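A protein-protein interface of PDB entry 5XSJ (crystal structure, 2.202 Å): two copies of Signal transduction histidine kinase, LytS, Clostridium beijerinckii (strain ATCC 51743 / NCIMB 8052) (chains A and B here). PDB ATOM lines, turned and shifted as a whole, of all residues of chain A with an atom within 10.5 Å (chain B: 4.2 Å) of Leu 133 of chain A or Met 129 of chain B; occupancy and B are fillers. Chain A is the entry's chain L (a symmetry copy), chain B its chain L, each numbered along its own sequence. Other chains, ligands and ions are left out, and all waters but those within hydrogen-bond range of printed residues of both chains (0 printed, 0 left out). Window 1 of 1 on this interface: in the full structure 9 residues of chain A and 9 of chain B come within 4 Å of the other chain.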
ATOM      1  N   SER A  14     -15.668 -13.475 -22.430  1.00  0.00           N
ATOM      2  CA  SER A  14     -15.882 -12.050 -22.580  1.00  0.00           C
ATOM      3  C   SER A  14     -17.256 -11.604 -22.133  1.00  0.00           C
ATOM      4  O   SER A  14     -17.367 -10.797 -21.246  1.00  0.00           O
ATOM      5  CB  SER A  14     -15.668 -11.603 -24.001  1.00  0.00           C
ATOM      6  OG  SER A  14     -15.874 -10.213 -24.099  1.00  0.00           O
ATOM      7  N   MET A  15     -18.293 -12.130 -22.761  1.00  0.00           N
ATOM      8  CA  MET A  15     -19.637 -11.888 -22.303  1.00  0.00           C
ATOM      9  C   MET A  15     -19.699 -12.424 -20.907  1.00  0.00           C
ATOM     10  O   MET A  15     -20.412 -11.886 -20.086  1.00  0.00           O
ATOM     11  CB  MET A  15     -20.664 -12.477 -23.256  1.00  0.00           C
ATOM     12  CG  MET A  15     -21.785 -11.521 -23.700  1.00  0.00           C
ATOM     13  SD  MET A  15     -21.253  -9.900 -24.684  1.00  0.00           S
ATOM     14  CE  MET A  15     -22.943  -8.931 -24.882  1.00  0.00           C
ATOM     15  N   LEU A  16     -18.930 -13.449 -20.612  1.00  0.00           N
ATOM     16  CA  LEU A  16     -18.807 -13.945 -19.260  1.00  0.00           C
ATOM     17  C   LEU A  16     -18.006 -13.024 -18.362  1.00  0.00           C
ATOM     18  O   LEU A  16     -18.293 -12.867 -17.207  1.00  0.00           O
ATOM     19  CB  LEU A  16     -18.142 -15.297 -19.281  1.00  0.00           C
ATOM     20  CG  LEU A  16     -17.795 -15.943 -17.956  1.00  0.00           C
ATOM     21  CD1 LEU A  16     -19.011 -16.650 -17.408  1.00  0.00           C
ATOM     22  CD2 LEU A  16     -16.680 -16.945 -18.136  1.00  0.00           C
ATOM     23  N   ASN A  17     -16.958 -12.457 -18.897  1.00  0.00           N
ATOM     24  CA  ASN A  17     -16.180 -11.451 -18.180  1.00  0.00           C
ATOM     25  C   ASN A  17     -17.010 -10.204 -17.868  1.00  0.00           C
ATOM     26  O   ASN A  17     -16.885  -9.616 -16.799  1.00  0.00           O
ATOM     27  CB  ASN A  17     -14.933 -11.076 -18.988  1.00  0.00           C
ATOM     28  CG  ASN A  17     -14.163  -9.935 -18.372  1.00  0.00           C
ATOM     29  OD1 ASN A  17     -13.548 -10.084 -17.310  1.00  0.00           O
ATOM     30  ND2 ASN A  17     -14.176  -8.780 -19.039  1.00  0.00           N
ATOM     31  N   ASN A  18     -17.871  -9.815 -18.799  1.00  0.00           N
ATOM     32  CA  ASN A  18     -18.767  -8.690 -18.581  1.00  0.00           C
ATOM     33  C   ASN A  18     -19.759  -8.926 -17.451  1.00  0.00           C
ATOM     34  O   ASN A  18     -20.099  -8.007 -16.708  1.00  0.00           O
ATOM     35  CB  ASN A  18     -19.525  -8.366 -19.861  1.00  0.00           C
ATOM     36  CG  ASN A  18     -18.668  -7.635 -20.860  1.00  0.00           C
ATOM     37  OD1 ASN A  18     -17.706  -6.965 -20.488  1.00  0.00           O
ATOM     38  ND2 ASN A  18     -19.015  -7.748 -22.134  1.00  0.00           N
ATOM     39  N   MET A  19     -20.221 -10.153 -17.291  1.00  0.00           N
ATOM     40  CA  MET A  19     -21.189 -10.360 -16.238  1.00  0.00           C
ATOM     41  C   MET A  19     -20.495 -10.690 -14.925  1.00  0.00           C
ATOM     42  O   MET A  19     -21.084 -10.538 -13.861  1.00  0.00           O
ATOM     43  CB  MET A  19     -22.214 -11.422 -16.637  1.00  0.00           C
ATOM     44  CG  MET A  19     -21.787 -12.851 -16.562  1.00  0.00           C
ATOM     45  SD  MET A  19     -23.239 -13.923 -17.383  1.00  0.00           S
ATOM     46  CE  MET A  19     -22.787 -13.661 -19.260  1.00  0.00           C
ATOM     47  N   LEU A  20     -19.236 -11.107 -14.988  1.00  0.00           N
ATOM     48  CA  LEU A  20     -18.432 -11.148 -13.772  1.00  0.00           C
ATOM     49  C   LEU A  20     -18.276  -9.737 -13.208  1.00  0.00           C
ATOM     50  O   LEU A  20     -18.443  -9.513 -12.008  1.00  0.00           O
ATOM     51  CB  LEU A  20     -17.057 -11.760 -14.034  1.00  0.00           C
ATOM     52  CG  LEU A  20     -17.018 -13.280 -14.171  1.00  0.00           C
ATOM     53  CD1 LEU A  20     -15.569 -13.756 -14.213  1.00  0.00           C
ATOM     54  CD2 LEU A  20     -17.771 -13.923 -13.016  1.00  0.00           C
ATOM     55  N   THR A  22     -20.153  -7.115 -13.849  1.00  0.00           N
ATOM     56  CA  THR A  22     -21.480  -6.649 -13.469  1.00  0.00           C
ATOM     57  C   THR A  22     -21.845  -7.192 -12.092  1.00  0.00           C
ATOM     58  O   THR A  22     -22.382  -6.472 -11.255  1.00  0.00           O
ATOM     59  CB  THR A  22     -22.529  -7.073 -14.518  1.00  0.00           C
ATOM     60  OG1 THR A  22     -22.271  -6.372 -15.738  1.00  0.00           O
ATOM     61  CG2 THR A  22     -23.934  -6.747 -14.056  1.00  0.00           C
ATOM     62  N   ASN A  23     -21.519  -8.453 -11.840  1.00  0.00           N
ATOM     63  CA  ASN A  23     -21.746  -9.005 -10.520  1.00  0.00           C
ATOM     64  C   ASN A  23     -20.843  -8.344  -9.465  1.00  0.00           C
ATOM     65  O   ASN A  23     -21.246  -8.165  -8.319  1.00  0.00           O
ATOM     66  CB  ASN A  23     -21.534 -10.516 -10.531  1.00  0.00           C
ATOM     67  CG  ASN A  23     -21.775 -11.142  -9.175  1.00  0.00           C
ATOM     68  OD1 ASN A  23     -22.887 -11.121  -8.662  1.00  0.00           O
ATOM     69  ND2 ASN A  23     -20.729 -11.703  -8.589  1.00  0.00           N
ATOM     70  N   GLU A  24     -19.626  -7.969  -9.844  1.00  0.00           N
ATOM     71  CA  GLU A  24     -18.735  -7.324  -8.893  1.00  0.00           C
ATOM     72  C   GLU A  24     -19.279  -5.964  -8.494  1.00  0.00           C
ATOM     73  O   GLU A  24     -19.233  -5.586  -7.329  1.00  0.00           O
ATOM     74  CB  GLU A  24     -17.320  -7.182  -9.475  1.00  0.00           C
ATOM     75  CG  GLU A  24     -16.519  -8.477  -9.406  1.00  0.00           C
ATOM     76  CD  GLU A  24     -15.261  -8.454 -10.272  1.00  0.00           C
ATOM     77  OE1 GLU A  24     -14.764  -7.354 -10.621  1.00  0.00           O
ATOM     78  OE2 GLU A  24     -14.769  -9.552 -10.597  1.00  0.00           O
ATOM     79  N   LYS A  26     -22.428  -5.016  -8.477  1.00  0.00           N
ATOM     80  CA  LYS A  26     -23.599  -5.222  -7.627  1.00  0.00           C
ATOM     81  C   LYS A  26     -23.179  -5.504  -6.186  1.00  0.00           C
ATOM     82  O   LYS A  26     -23.729  -4.929  -5.251  1.00  0.00           O
ATOM     83  CB  LYS A  26     -24.449  -6.365  -8.190  1.00  0.00           C
ATOM     84  CG  LYS A  26     -25.802  -6.552  -7.518  1.00  0.00           C
ATOM     85  CD  LYS A  26     -26.586  -7.660  -8.204  1.00  0.00           C
ATOM     86  CE  LYS A  26     -27.976  -7.771  -7.589  1.00  0.00           C
ATOM     87  NZ  LYS A  26     -27.877  -7.620  -6.098  1.00  0.00           N
ATOM     88  N   GLN A  27     -22.182  -6.365  -6.011  1.00  0.00           N
ATOM     89  CA  GLN A  27     -21.622  -6.626  -4.685  1.00  0.00           C
ATOM     90  C   GLN A  27     -21.013  -5.364  -4.057  1.00  0.00           C
ATOM     91  O   GLN A  27     -21.176  -5.117  -2.855  1.00  0.00           O
ATOM     92  CB  GLN A  27     -20.544  -7.701  -4.751  1.00  0.00           C
ATOM     93  CG  GLN A  27     -20.952  -9.046  -5.320  1.00  0.00           C
ATOM     94  CD  GLN A  27     -19.798 -10.064  -5.226  1.00  0.00           C
ATOM     95  OE1 GLN A  27     -18.624  -9.751  -5.518  1.00  0.00           O
ATOM     96  NE2 GLN A  27     -20.128 -11.279  -4.796  1.00  0.00           N
ATOM     97  N   ASP A  70     -22.303  -1.539 -26.058  1.00  0.00           N
ATOM     98  CA  ASP A  70     -22.964  -1.515 -27.366  1.00  0.00           C
ATOM     99  C   ASP A  70     -24.146  -0.542 -27.374  1.00  0.00           C
ATOM    100  O   ASP A  70     -24.249   0.312 -26.500  1.00  0.00           O
ATOM    101  CB  ASP A  70     -23.433  -2.919 -27.768  1.00  0.00           C
ATOM    102  CG  ASP A  70     -24.416  -3.525 -26.774  1.00  0.00           C
ATOM    103  OD1 ASP A  70     -24.058  -4.539 -26.131  1.00  0.00           O
ATOM    104  OD2 ASP A  70     -25.546  -2.995 -26.636  1.00  0.00           O
ATOM    105  N   ASN A  73     -26.912  -1.615 -24.047  1.00  0.00           N
ATOM    106  CA  ASN A  73     -26.368  -1.553 -22.696  1.00  0.00           C
ATOM    107  C   ASN A  73     -25.893  -0.156 -22.336  1.00  0.00           C
ATOM    108  O   ASN A  73     -25.846   0.208 -21.174  1.00  0.00           O
ATOM    109  CB  ASN A  73     -25.219  -2.541 -22.529  1.00  0.00           C
ATOM    110  CG  ASN A  73     -25.666  -3.978 -22.642  1.00  0.00           C
ATOM    111  OD1 ASN A  73     -26.839  -4.304 -22.424  1.00  0.00           O
ATOM    112  ND2 ASN A  73     -24.726  -4.857 -22.979  1.00  0.00           N
ATOM    113  N   ALA A 125     -28.197  -3.503 -12.374  1.00  0.00           N
ATOM    114  CA  ALA A 125     -27.121  -4.480 -12.431  1.00  0.00           C
ATOM    115  C   ALA A 125     -27.639  -5.852 -12.830  1.00  0.00           C
ATOM    116  O   ALA A 125     -27.038  -6.529 -13.647  1.00  0.00           O
ATOM    117  CB  ALA A 125     -26.409  -4.558 -11.092  1.00  0.00           C
ATOM    118  N   SER A 126     -28.765  -6.263 -12.258  1.00  0.00           N
ATOM    119  CA  SER A 126     -29.294  -7.578 -12.588  1.00  0.00           C
ATOM    120  C   SER A 126     -29.841  -7.564 -14.020  1.00  0.00           C
ATOM    121  O   SER A 126     -29.753  -8.560 -14.727  1.00  0.00           O
ATOM    122  CB  SER A 126     -30.364  -8.001 -11.586  1.00  0.00           C
ATOM    123  OG  SER A 126     -31.625  -7.542 -12.015  1.00  0.00           O
ATOM    124  N   THR A 127     -30.368  -6.426 -14.465  1.00  0.00           N
ATOM    125  CA  THR A 127     -30.766  -6.280 -15.868  1.00  0.00           C
ATOM    126  C   THR A 127     -29.563  -6.408 -16.800  1.00  0.00           C
ATOM    127  O   THR A 127     -29.615  -7.111 -17.814  1.00  0.00           O
ATOM    128  CB  THR A 127     -31.447  -4.927 -16.131  1.00  0.00           C
ATOM    129  OG1 THR A 127     -32.682  -4.854 -15.412  1.00  0.00           O
ATOM    130  CG2 THR A 127     -31.719  -4.741 -17.608  1.00  0.00           C
ATOM    131  N   LEU A 128     -28.477  -5.719 -16.462  1.00  0.00           N
ATOM    132  CA  LEU A 128     -27.255  -5.829 -17.245  1.00  0.00           C
ATOM    133  C   LEU A 128     -26.778  -7.271 -17.319  1.00  0.00           C
ATOM    134  O   LEU A 128     -26.422  -7.759 -18.385  1.00  0.00           O
ATOM    135  CB  LEU A 128     -26.160  -4.954 -16.655  1.00  0.00           C
ATOM    136  CG  LEU A 128     -26.122  -3.532 -17.199  1.00  0.00           C
ATOM    137  CD1 LEU A 128     -25.067  -2.726 -16.444  1.00  0.00           C
ATOM    138  CD2 LEU A 128     -25.841  -3.529 -18.696  1.00  0.00           C
ATOM    139  N   MET A 129     -26.786  -7.952 -16.178  1.00  0.00           N
ATOM    140  CA  MET A 129     -26.265  -9.313 -16.107  1.00  0.00           C
ATOM    141  C   MET A 129     -27.064 -10.242 -17.001  1.00  0.00           C
ATOM    142  O   MET A 129     -26.513 -11.143 -17.627  1.00  0.00           O
ATOM    143  CB  MET A 129     -26.280  -9.826 -14.670  1.00  0.00           C
ATOM    144  CG  MET A 129     -25.103 -10.723 -14.301  1.00  0.00           C
ATOM    145  SD  MET A 129     -25.124 -11.112 -12.533  1.00  0.00           S
ATOM    146  CE  MET A 129     -25.322  -9.477 -11.825  1.00  0.00           C
ATOM    147  N   GLN A 130     -28.370 -10.014 -17.060  1.00  0.00           N
ATOM    148  CA  GLN A 130     -29.234 -10.792 -17.930  1.00  0.00           C
ATOM    149  C   GLN A 130     -28.935 -10.531 -19.399  1.00  0.00           C
ATOM    150  O   GLN A 130     -28.923 -11.461 -20.205  1.00  0.00           O
ATOM    151  CB  GLN A 130     -30.705 -10.496 -17.649  1.00  0.00           C
ATOM    152  CG  GLN A 130     -31.190 -10.917 -16.272  1.00  0.00           C
ATOM    153  CD  GLN A 130     -32.694 -10.710 -16.126  1.00  0.00           C
ATOM    154  OE1 GLN A 130     -33.492 -11.289 -16.880  1.00  0.00           O
ATOM    155  NE2 GLN A 130     -33.086  -9.870 -15.172  1.00  0.00           N
ATOM    156  N   ASN A 131     -28.704  -9.269 -19.744  1.00  0.00           N
ATOM    157  CA  ASN A 131     -28.368  -8.900 -21.114  1.00  0.00           C
ATOM    158  C   ASN A 131     -27.053  -9.503 -21.587  1.00  0.00           C
ATOM    159  O   ASN A 131     -26.958  -9.996 -22.707  1.00  0.00           O
ATOM    160  CB  ASN A 131     -28.314  -7.385 -21.247  1.00  0.00           C
ATOM    161  CG  ASN A 131     -29.678  -6.759 -21.148  1.00  0.00           C
ATOM    162  OD1 ASN A 131     -30.667  -7.442 -20.880  1.00  0.00           O
ATOM    163  ND2 ASN A 131     -29.744  -5.451 -21.365  1.00  0.00           N
ATOM    164  N   PHE A 132     -26.033  -9.449 -20.734  1.00  0.00           N
ATOM    165  CA  PHE A 132     -24.767 -10.101 -21.033  1.00  0.00           C
ATOM    166  C   PHE A 132     -24.946 -11.612 -21.163  1.00  0.00           C
ATOM    167  O   PHE A 132     -24.279 -12.260 -21.963  1.00  0.00           O
ATOM    168  CB  PHE A 132     -23.736  -9.791 -19.949  1.00  0.00           C
ATOM    169  CG  PHE A 132     -23.219  -8.388 -19.996  1.00  0.00           C
ATOM    170  CD1 PHE A 132     -22.867  -7.804 -21.203  1.00  0.00           C
ATOM    171  CD2 PHE A 132     -23.096  -7.650 -18.835  1.00  0.00           C
ATOM    172  CE1 PHE A 132     -22.387  -6.506 -21.247  1.00  0.00           C
ATOM    173  CE2 PHE A 132     -22.616  -6.355 -18.869  1.00  0.00           C
ATOM    174  CZ  PHE A 132     -22.262  -5.780 -20.077  1.00  0.00           C
ATOM    175  N   LEU A 133     -25.856 -12.165 -20.370  1.00  0.00           N
ATOM    176  CA  LEU A 133     -26.114 -13.595 -20.391  1.00  0.00           C
ATOM    177  C   LEU A 133     -26.702 -14.032 -21.730  1.00  0.00           C
ATOM    178  O   LEU A 133     -26.583 -15.188 -22.108  1.00  0.00           O
ATOM    179  CB  LEU A 133     -27.054 -13.979 -19.246  1.00  0.00           C
ATOM    180  CG  LEU A 133     -27.207 -15.454 -18.878  1.00  0.00           C
ATOM    181  CD1 LEU A 133     -25.856 -16.090 -18.611  1.00  0.00           C
ATOM    182  CD2 LEU A 133     -28.080 -15.578 -17.650  1.00  0.00           C
ATOM    183  N   GLU A 134     -27.288 -13.089 -22.461  1.00  0.00           N
ATOM    184  CA  GLU A 134     -28.075 -13.410 -23.644  1.00  0.00           C
ATOM    185  C   GLU A 134     -27.444 -12.982 -24.975  1.00  0.00           C
ATOM    186  O   GLU A 134     -28.086 -12.292 -25.772  1.00  0.00           O
ATOM    187  CB  GLU A 134     -29.462 -12.774 -23.509  1.00  0.00           C
ATOM    188  CG  GLU A 134     -30.276 -13.343 -22.356  1.00  0.00           C
ATOM    189  CD  GLU A 134     -31.458 -12.471 -21.969  1.00  0.00           C
ATOM    190  OE1 GLU A 134     -31.674 -11.430 -22.629  1.00  0.00           O
ATOM    191  OE2 GLU A 134     -32.172 -12.827 -21.002  1.00  0.00           O
ATOM    192  N   ALA A 135     -26.202 -13.397 -25.220  1.00  0.00           N
ATOM    193  CA  ALA A 135     -25.565 -13.190 -26.524  1.00  0.00           C
ATOM    194  C   ALA A 135     -26.052 -14.227 -27.547  1.00  0.00           C
ATOM    195  O   ALA A 135     -25.414 -15.264 -27.771  1.00  0.00           O
ATOM    196  CB  ALA A 135     -24.049 -13.243 -26.393  1.00  0.00           C
ATOM    197  N   MET B  19     -27.206 -21.212 -14.810  1.00  0.00           N
ATOM    198  CA  MET B  19     -27.670 -19.846 -14.724  1.00  0.00           C
ATOM    199  C   MET B  19     -28.436 -19.456 -15.979  1.00  0.00           C
ATOM    200  O   MET B  19     -29.208 -18.505 -15.959  1.00  0.00           O
ATOM    201  CB  MET B  19     -26.511 -18.892 -14.431  1.00  0.00           C
ATOM    202  CG  MET B  19     -25.605 -18.542 -15.566  1.00  0.00           C
ATOM    203  SD  MET B  19     -24.093 -17.520 -14.794  1.00  0.00           S
ATOM    204  CE  MET B  19     -23.031 -19.009 -14.122  1.00  0.00           C
ATOM    205  N   LEU B  20     -28.257 -20.205 -17.061  1.00  0.00           N
ATOM    206  CA  LEU B  20     -29.175 -20.072 -18.185  1.00  0.00           C
ATOM    207  C   LEU B  20     -30.585 -20.466 -17.751  1.00  0.00           C
ATOM    208  O   LEU B  20     -31.556 -19.768 -18.045  1.00  0.00           O
ATOM    209  CB  LEU B  20     -28.733 -20.931 -19.369  1.00  0.00           C
ATOM    210  CG  LEU B  20     -27.567 -20.387 -20.191  1.00  0.00           C
ATOM    211  CD1 LEU B  20     -27.385 -21.232 -21.448  1.00  0.00           C
ATOM    212  CD2 LEU B  20     -27.820 -18.929 -20.546  1.00  0.00           C
ATOM    213  N   THR B  22     -31.757 -20.617 -14.684  1.00  0.00           N
ATOM    214  CA  THR B  22     -32.183 -19.663 -13.669  1.00  0.00           C
ATOM    215  C   THR B  22     -32.710 -18.398 -14.336  1.00  0.00           C
ATOM    216  O   THR B  22     -33.733 -17.853 -13.931  1.00  0.00           O
ATOM    217  CB  THR B  22     -31.021 -19.331 -12.710  1.00  0.00           C
ATOM    218  OG1 THR B  22     -30.701 -20.500 -11.948  1.00  0.00           O
ATOM    219  CG2 THR B  22     -31.396 -18.216 -11.756  1.00  0.00           C
ATOM    220  N   ASN B  23     -32.034 -17.949 -15.385  1.00  0.00           N
ATOM    221  CA  ASN B  23     -32.532 -16.809 -16.128  1.00  0.00           C
ATOM    222  C   ASN B  23     -33.847 -17.135 -16.854  1.00  0.00           C
ATOM    223  O   ASN B  23     -34.720 -16.282 -16.986  1.00  0.00           O
ATOM    224  CB  ASN B  23     -31.482 -16.320 -17.121  1.00  0.00           C
ATOM    225  CG  ASN B  23     -31.951 -15.119 -17.913  1.00  0.00           C
ATOM    226  OD1 ASN B  23     -32.182 -14.052 -17.356  1.00  0.00           O
ATOM    227  ND2 ASN B  23     -32.095 -15.290 -19.217  1.00  0.00           N
ATOM    228  N   ALA B 125     -34.320 -15.636  -7.716  1.00  0.00           N
ATOM    229  CA  ALA B 125     -33.725 -16.013  -8.989  1.00  0.00           C
ATOM    230  C   ALA B 125     -32.412 -15.286  -9.224  1.00  0.00           C
ATOM    231  O   ALA B 125     -31.440 -15.882  -9.657  1.00  0.00           O
ATOM    232  CB  ALA B 125     -34.691 -15.730 -10.126  1.00  0.00           C
ATOM    233  N   SER B 126     -32.376 -13.992  -8.928  1.00  0.00           N
ATOM    234  CA  SER B 126     -31.149 -13.241  -9.154  1.00  0.00           C
ATOM    235  C   SER B 126     -30.094 -13.666  -8.125  1.00  0.00           C
ATOM    236  O   SER B 126     -28.909 -13.702  -8.431  1.00  0.00           O
ATOM    237  CB  SER B 126     -31.411 -11.740  -9.095  1.00  0.00           C
ATOM    238  OG  SER B 126     -31.277 -11.285  -7.768  1.00  0.00           O
ATOM    239  N   THR B 127     -30.523 -14.030  -6.920  1.00  0.00           N
ATOM    240  CA  THR B 127     -29.602 -14.601  -5.934  1.00  0.00           C
ATOM    241  C   THR B 127     -29.015 -15.923  -6.426  1.00  0.00           C
ATOM    242  O   THR B 127     -27.805 -16.157  -6.333  1.00  0.00           O
ATOM    243  CB  THR B 127     -30.290 -14.845  -4.581  1.00  0.00           C
ATOM    244  OG1 THR B 127     -30.684 -13.597  -4.002  1.00  0.00           O
ATOM    245  CG2 THR B 127     -29.360 -15.564  -3.627  1.00  0.00           C
ATOM    246  N   LEU B 128     -29.875 -16.795  -6.944  1.00  0.00           N
ATOM    247  CA  LEU B 128     -29.408 -18.054  -7.505  1.00  0.00           C
ATOM    248  C   LEU B 128     -28.396 -17.817  -8.616  1.00  0.00           C
ATOM    249  O   LEU B 128     -27.354 -18.462  -8.662  1.00  0.00           O
ATOM    250  CB  LEU B 128     -30.576 -18.869  -8.037  1.00  0.00           C
ATOM    251  CG  LEU B 128     -31.208 -19.809  -7.020  1.00  0.00           C
ATOM    252  CD1 LEU B 128     -32.437 -20.475  -7.636  1.00  0.00           C
ATOM    253  CD2 LEU B 128     -30.205 -20.853  -6.544  1.00  0.00           C
ATOM    254  N   MET B 129     -28.706 -16.879  -9.503  1.00  0.00           N
ATOM    255  CA  MET B 129     -27.859 -16.627 -10.664  1.00  0.00           C
ATOM    256  C   MET B 129     -26.478 -16.168 -10.232  1.00  0.00           C
ATOM    257  O   MET B 129     -25.475 -16.526 -10.843  1.00  0.00           O
ATOM    258  CB  MET B 129     -28.494 -15.588 -11.585  1.00  0.00           C
ATOM    259  CG  MET B 129     -28.263 -15.830 -13.073  1.00  0.00           C
ATOM    260  SD  MET B 129     -29.214 -14.654 -14.067  1.00  0.00           S
ATOM    261  CE  MET B 129     -30.838 -14.812 -13.325  1.00  0.00           C
ATOM    262  N   GLN B 130     -26.433 -15.375  -9.170  1.00  0.00           N
ATOM    263  CA  GLN B 130     -25.168 -14.921  -8.619  1.00  0.00           C
ATOM    264  C   GLN B 130     -24.370 -16.072  -8.023  1.00  0.00           C
ATOM    265  O   GLN B 130     -23.153 -16.137  -8.195  1.00  0.00           O
ATOM    266  CB  GLN B 130     -25.387 -13.849  -7.555  1.00  0.00           C
ATOM    267  CG  GLN B 130     -25.986 -12.551  -8.070  1.00  0.00           C
ATOM    268  CD  GLN B 130     -26.043 -11.493  -6.973  1.00  0.00           C
ATOM    269  OE1 GLN B 130     -25.007 -11.105  -6.407  1.00  0.00           O
ATOM    270  NE2 GLN B 130     -27.250 -11.036  -6.653  1.00  0.00           N
ATOM    271  N   ASN B 131     -25.053 -16.968  -7.319  1.00  0.00           N
ATOM    272  CA  ASN B 131     -24.404 -18.135  -6.733  1.00  0.00           C
ATOM    273  C   ASN B 131     -23.815 -19.075  -7.776  1.00  0.00           C
ATOM    274  O   ASN B 131     -22.699 -19.562  -7.619  1.00  0.00           O
ATOM    275  CB  ASN B 131     -25.389 -18.894  -5.858  1.00  0.00           C
ATOM    276  CG  ASN B 131     -25.729 -18.141  -4.601  1.00  0.00           C
ATOM    277  OD1 ASN B 131     -25.307 -16.998  -4.417  1.00  0.00           O
ATOM    278  ND2 ASN B 131     -26.495 -18.774  -3.722  1.00  0.00           N
ATOM    279  N   PHE B 132     -24.575 -19.339  -8.835  1.00  0.00           N
ATOM    280  CA  PHE B 132     -24.067 -20.125  -9.949  1.00  0.00           C
ATOM    281  C   PHE B 132     -22.884 -19.427 -10.617  1.00  0.00           C
ATOM    282  O   PHE B 132     -21.953 -20.073 -11.089  1.00  0.00           O
ATOM    283  CB  PHE B 132     -25.170 -20.376 -10.975  1.00  0.00           C
ATOM    284  CG  PHE B 132     -26.196 -21.367 -10.524  1.00  0.00           C
ATOM    285  CD1 PHE B 132     -25.814 -22.545  -9.900  1.00  0.00           C
ATOM    286  CD2 PHE B 132     -27.541 -21.116 -10.712  1.00  0.00           C
ATOM    287  CE1 PHE B 132     -26.763 -23.464  -9.483  1.00  0.00           C
ATOM    288  CE2 PHE B 132     -28.493 -22.027 -10.301  1.00  0.00           C
ATOM    289  CZ  PHE B 132     -28.105 -23.202  -9.684  1.00  0.00           C
ATOM    290  N   LEU B 133     -22.928 -18.100 -10.650  1.00  0.00           N
ATOM    291  CA  LEU B 133     -21.869 -17.319 -11.267  1.00  0.00           C
ATOM    292  C   LEU B 133     -20.555 -17.472 -10.507  1.00  0.00           C
ATOM    293  O   LEU B 133     -19.489 -17.274 -11.071  1.00  0.00           O
ATOM    294  CB  LEU B 133     -22.275 -15.845 -11.341  1.00  0.00           C
ATOM    295  CG  LEU B 133     -21.468 -14.901 -12.231  1.00  0.00           C
ATOM    296  CD1 LEU B 133     -21.374 -15.434 -13.646  1.00  0.00           C
ATOM    297  CD2 LEU B 133     -22.123 -13.539 -12.242  1.00  0.00           C
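Leu 133 of chain A touches four residues of chain B.
Met 129 of chain B touches just one residue of chain A: Leu 133 (3.9 Å).
Of chain A, only Leu 133 comes within 4 Å of Leu 20 of chain B.
Of chain A, only Gln 130 (3.1 Å), Leu 133 (3.5 Å) and Glu 134 (3.0 Å) come within 4 Å of Asn 23 of chain B.
No residue of chain A comes within 4 Å of Ala 125 of chain B.
Of the printed residues of chain A, Gln 130 of chain B touches Asn 23 (3.1 Å) and Lys 26 (3.5 Å).
Of the printed residues of chain B, Gln 130 of chain A touches Asn 23 (3.1 Å).
Of the printed residues of chain B, Asn 23 of chain A touches Gln 130 (3.1 Å) and Leu 133 (3.5 Å).
Of the printed residues of chain B, Lys 26 of chain A touches Gln 130.
Asn 17 of chain A touches none of the printed residues of chain B.
The nearest printed residue of chain B that does not touch Leu 133 of chain A is Thr 22 of chain B (6.4 Å).
The nearest printed residue of chain A that does not touch Gln 130 of chain B is Gln 27 of chain A (4.7 Å).
Met 19 of chain A touches Leu 133 of chain B, and with the chains exchanged Leu 133 of chain A touches Met 19 of chain B.
Leu 20 of chain A touches Leu 133 of chain B, and with the chains exchanged Leu 133 of chain A touches Leu 20 of chain B.
Asn 23 of chain A touches Leu 133 of chain B, and with the chains exchanged Leu 133 of chain A touches Asn 23 of chain B.
Met 129 of chain A touches Leu 133 of chain B, and with the chains exchanged Leu 133 of chain A touches Met 129 of chain B.
13 positions are printed for both chains.
Of the 12 pairs that touch across the chains among the printed residues, 10 have their exchanged pair printed and touching as well.
OE1 of Gln 130 of chain A sits close to OD1 of Asn 23 of chain B, at 3.1 Å.
OE2 of Glu 134 of chain A is in hydrogen-bond range of ND2 of Asn 23 of chain B (3.0 Å).
OD1 of Asn 23 of chain A sits close to OE1 of Gln 130 of chain B, at 3.1 Å.
Printed residues of chain B that touch a printed residue of chain A: Met 19, Leu 20, Asn 23, Met 129, Gln 130 and Leu 133.
Hydrophobic or aromatic side chains of chain B that line the printed part of chain A: Met 19, Leu 20, Met 129 and Leu 133.
Of the 25 printed residues of chain A, 8 touch a printed residue of chain B.
Hydrophobic or aromatic side chains of chain A that line the printed part of chain B: Met 19, Leu 20, Met 129 and Leu 133.
Among the printed residues, merely in contact across the chains: Met 19 of chain A with Leu 133 of chain B, Leu 20 of chain A with Leu 133 of chain B, Asn 23 of chain A with Leu 133 of chain B, Lys 26 of chain A with Gln 130 of chain B, Met 129 of chain A with Leu 133 of chain B, Leu 133 of chain A with Met 19 of chain B, Leu 133 of chain A with Leu 20 of chain B, Leu 133 of chain A with Asn 23 of chain B and Leu 133 of chain A with Met 129 of chain B.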
